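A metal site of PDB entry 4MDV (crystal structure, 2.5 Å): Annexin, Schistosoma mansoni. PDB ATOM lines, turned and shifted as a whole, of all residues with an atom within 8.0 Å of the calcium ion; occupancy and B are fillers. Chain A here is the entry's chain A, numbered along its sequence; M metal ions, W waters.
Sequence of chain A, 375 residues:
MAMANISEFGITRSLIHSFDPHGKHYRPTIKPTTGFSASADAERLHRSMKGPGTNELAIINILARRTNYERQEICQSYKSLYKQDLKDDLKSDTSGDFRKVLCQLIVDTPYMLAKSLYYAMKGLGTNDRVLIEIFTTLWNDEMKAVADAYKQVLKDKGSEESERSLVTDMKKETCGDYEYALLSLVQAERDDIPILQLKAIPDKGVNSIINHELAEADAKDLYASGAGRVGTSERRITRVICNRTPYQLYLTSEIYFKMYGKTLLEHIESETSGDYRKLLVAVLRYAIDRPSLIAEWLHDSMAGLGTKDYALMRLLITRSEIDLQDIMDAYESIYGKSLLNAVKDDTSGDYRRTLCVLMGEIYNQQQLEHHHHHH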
ATOM      1  N   HIS A  46      12.511 -24.389  28.934  1.00  0.00           N
ATOM      2  CA  HIS A  46      11.734 -24.219  27.701  1.00  0.00           C
ATOM      3  C   HIS A  46      10.268 -23.973  28.027  1.00  0.00           C
ATOM      4  O   HIS A  46       9.628 -23.076  27.461  1.00  0.00           O
ATOM      5  CB  HIS A  46      11.803 -25.457  26.817  1.00  0.00           C
ATOM      6  CG  HIS A  46      10.616 -25.597  25.917  1.00  0.00           C
ATOM      7  ND1 HIS A  46       9.492 -26.310  26.272  1.00  0.00           N
ATOM      8  CD2 HIS A  46      10.359 -25.073  24.692  1.00  0.00           C
ATOM      9  CE1 HIS A  46       8.600 -26.239  25.305  1.00  0.00           C
ATOM     10  NE2 HIS A  46       9.097 -25.496  24.331  1.00  0.00           N
ATOM     11  N   ARG A  47       9.735 -24.801  28.909  1.00  0.00           N
ATOM     12  CA  ARG A  47       8.383 -24.667  29.391  1.00  0.00           C
ATOM     13  C   ARG A  47       8.169 -23.238  29.864  1.00  0.00           C
ATOM     14  O   ARG A  47       7.216 -22.575  29.458  1.00  0.00           O
ATOM     15  CB  ARG A  47       8.161 -25.661  30.528  1.00  0.00           C
ATOM     16  CG  ARG A  47       6.952 -25.412  31.408  1.00  0.00           C
ATOM     17  CD  ARG A  47       6.573 -26.679  32.208  1.00  0.00           C
ATOM     18  NE  ARG A  47       7.736 -27.510  32.551  1.00  0.00           N
ATOM     19  CZ  ARG A  47       8.014 -28.670  31.986  1.00  0.00           C
ATOM     20  NH1 ARG A  47       7.210 -29.157  31.049  1.00  0.00           N
ATOM     21  NH2 ARG A  47       9.088 -29.373  32.353  1.00  0.00           N
ATOM     22  N   SER A  48       9.093 -22.756  30.693  1.00  0.00           N
ATOM     23  CA  SER A  48       8.919 -21.477  31.372  1.00  0.00           C
ATOM     24  C   SER A  48       8.873 -20.266  30.452  1.00  0.00           C
ATOM     25  O   SER A  48       8.559 -19.156  30.904  1.00  0.00           O
ATOM     26  CB  SER A  48       9.928 -21.299  32.500  1.00  0.00           C
ATOM     27  OG  SER A  48       9.489 -22.046  33.620  1.00  0.00           O
ATOM     28  N   MET A  49       9.157 -20.489  29.170  1.00  0.00           N
ATOM     29  CA  MET A  49       9.102 -19.437  28.171  1.00  0.00           C
ATOM     30  C   MET A  49       7.876 -19.561  27.251  1.00  0.00           C
ATOM     31  O   MET A  49       7.643 -18.709  26.386  1.00  0.00           O
ATOM     32  CB  MET A  49      10.413 -19.427  27.384  1.00  0.00           C
ATOM     33  CG  MET A  49      11.600 -19.055  28.261  1.00  0.00           C
ATOM     34  SD  MET A  49      13.150 -18.924  27.352  1.00  0.00           S
ATOM     35  CE  MET A  49      13.649 -20.645  27.261  1.00  0.00           C
ATOM     36  N   LYS A  50       7.090 -20.609  27.465  1.00  0.00           N
ATOM     37  CA  LYS A  50       5.853 -20.787  26.713  1.00  0.00           C
ATOM     38  C   LYS A  50       4.877 -19.664  27.048  1.00  0.00           C
ATOM     39  O   LYS A  50       5.022 -18.987  28.063  1.00  0.00           O
ATOM     40  N   GLY A  51       3.896 -19.467  26.182  1.00  0.00           N
ATOM     41  CA  GLY A  51       2.907 -18.426  26.387  1.00  0.00           C
ATOM     42  C   GLY A  51       3.415 -17.075  25.944  1.00  0.00           C
ATOM     43  O   GLY A  51       4.571 -16.942  25.536  1.00  0.00           O
ATOM     44  N   PRO A  52       2.558 -16.046  26.021  1.00  0.00           N
ATOM     45  CA  PRO A  52       2.877 -14.672  25.631  1.00  0.00           C
ATOM     46  C   PRO A  52       3.872 -14.037  26.593  1.00  0.00           C
ATOM     47  O   PRO A  52       4.640 -13.142  26.226  1.00  0.00           O
ATOM     48  CB  PRO A  52       1.521 -13.962  25.777  1.00  0.00           C
ATOM     49  CG  PRO A  52       0.847 -14.708  26.884  1.00  0.00           C
ATOM     50  CD  PRO A  52       1.236 -16.147  26.668  1.00  0.00           C
ATOM     51  N   GLY A  53       3.822 -14.500  27.845  1.00  0.00           N
ATOM     52  CA  GLY A  53       4.679 -13.972  28.887  1.00  0.00           C
ATOM     53  C   GLY A  53       5.785 -14.934  29.298  1.00  0.00           C
ATOM     54  O   GLY A  53       6.202 -15.822  28.536  1.00  0.00           O
ATOM     55  N   THR A  54       6.274 -14.748  30.519  1.00  0.00           N
ATOM     56  CA  THR A  54       7.404 -15.535  30.969  1.00  0.00           C
ATOM     57  C   THR A  54       7.362 -15.766  32.465  1.00  0.00           C
ATOM     58  O   THR A  54       6.957 -14.894  33.241  1.00  0.00           O
ATOM     59  CB  THR A  54       8.741 -14.876  30.624  1.00  0.00           C
ATOM     60  OG1 THR A  54       9.017 -15.085  29.233  1.00  0.00           O
ATOM     61  CG2 THR A  54       9.858 -15.469  31.471  1.00  0.00           C
ATOM     62  N   ASN A  55       7.790 -16.962  32.839  1.00  0.00           N
ATOM     63  CA  ASN A  55       7.939 -17.357  34.227  1.00  0.00           C
ATOM     64  C   ASN A  55       9.367 -17.068  34.648  1.00  0.00           C
ATOM     65  O   ASN A  55      10.233 -17.963  34.654  1.00  0.00           O
ATOM     66  CB  ASN A  55       7.603 -18.841  34.389  1.00  0.00           C
ATOM     67  CG  ASN A  55       7.367 -19.252  35.838  1.00  0.00           C
ATOM     68  OD1 ASN A  55       8.027 -18.769  36.772  1.00  0.00           O
ATOM     69  ND2 ASN A  55       6.414 -20.158  36.030  1.00  0.00           N
ATOM     70  N   ASP A  89      16.665 -17.791  22.871  1.00  0.00           N
ATOM     71  CA  ASP A  89      15.320 -17.926  23.410  1.00  0.00           C
ATOM     72  C   ASP A  89      15.120 -17.126  24.704  1.00  0.00           C
ATOM     73  O   ASP A  89      14.025 -16.625  24.984  1.00  0.00           O
ATOM     74  CB  ASP A  89      14.935 -19.398  23.610  1.00  0.00           C
ATOM     75  CG  ASP A  89      14.551 -20.093  22.293  1.00  0.00           C
ATOM     76  OD1 ASP A  89      13.967 -19.408  21.410  1.00  0.00           O
ATOM     77  OD2 ASP A  89      14.851 -21.313  22.145  1.00  0.00           O
ATOM     78  N   SER A  92      15.039 -13.233  23.759  1.00  0.00           N
ATOM     79  CA  SER A  92      13.808 -12.771  23.140  1.00  0.00           C
ATOM     80  C   SER A  92      12.623 -12.843  24.097  1.00  0.00           C
ATOM     81  O   SER A  92      11.585 -12.189  23.883  1.00  0.00           O
ATOM     82  CB  SER A  92      13.536 -13.542  21.834  1.00  0.00           C
ATOM     83  OG  SER A  92      13.378 -14.928  22.054  1.00  0.00           O
ATOM     84  N   ASP A  93      12.790 -13.601  25.171  1.00  0.00           N
ATOM     85  CA  ASP A  93      11.755 -13.689  26.216  1.00  0.00           C
ATOM     86  C   ASP A  93      11.913 -12.707  27.374  1.00  0.00           C
ATOM     87  O   ASP A  93      11.006 -12.566  28.203  1.00  0.00           O
ATOM     88  CB  ASP A  93      11.673 -15.116  26.762  1.00  0.00           C
ATOM     89  CG  ASP A  93      10.474 -15.865  26.233  1.00  0.00           C
ATOM     90  OD1 ASP A  93      10.550 -16.378  25.083  1.00  0.00           O
ATOM     91  OD2 ASP A  93       9.451 -15.924  26.942  1.00  0.00           O
ATOM     92  N   THR A  94      13.033 -12.005  27.427  1.00  0.00           N
ATOM     93  CA  THR A  94      13.273 -11.089  28.524  1.00  0.00           C
ATOM     94  C   THR A  94      13.816  -9.742  28.007  1.00  0.00           C
ATOM     95  O   THR A  94      14.048  -9.587  26.801  1.00  0.00           O
ATOM     96  CB  THR A  94      14.218 -11.762  29.555  1.00  0.00           C
ATOM     97  OG1 THR A  94      15.573 -11.765  29.072  1.00  0.00           O
ATOM     98  CG2 THR A  94      13.770 -13.212  29.782  1.00  0.00           C
HETATM   99 CA    CA M   1       7.192 -16.278  26.263  1.00  0.00          CA
HETATM  100  O   HOH W   1       7.617 -17.143  23.784  1.00  0.00           O
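The backbone carbonyl oxygen of Asp 93 sits at hydrogen-bond distance from the side-chain hydroxyl of Thr 54, at 3.4 Å.
Lys 50 touches the calcium ion. Thr 54 touches the calcium ion (OG1 to CA, 3.7 Å). Six residues have an atom within 4 Å of the calcium ion: Met 49, Lys 50, Gly 51, Gly 53, Thr 54 and Asp 93.
OD2 of Asp 93 is bound to the calcium ion. The calcium ion is bound by O of Met 49, 2.5 Å away. The calcium ion is bound by the backbone carbonyl oxygen (O) of Gly 53. Water W1 binds the calcium ion (2.7 Å). The calcium ion is bound by the backbone carbonyl oxygen (O) of Gly 51 (2.8 Å). The calcium ion has five donor atoms within binding distance.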
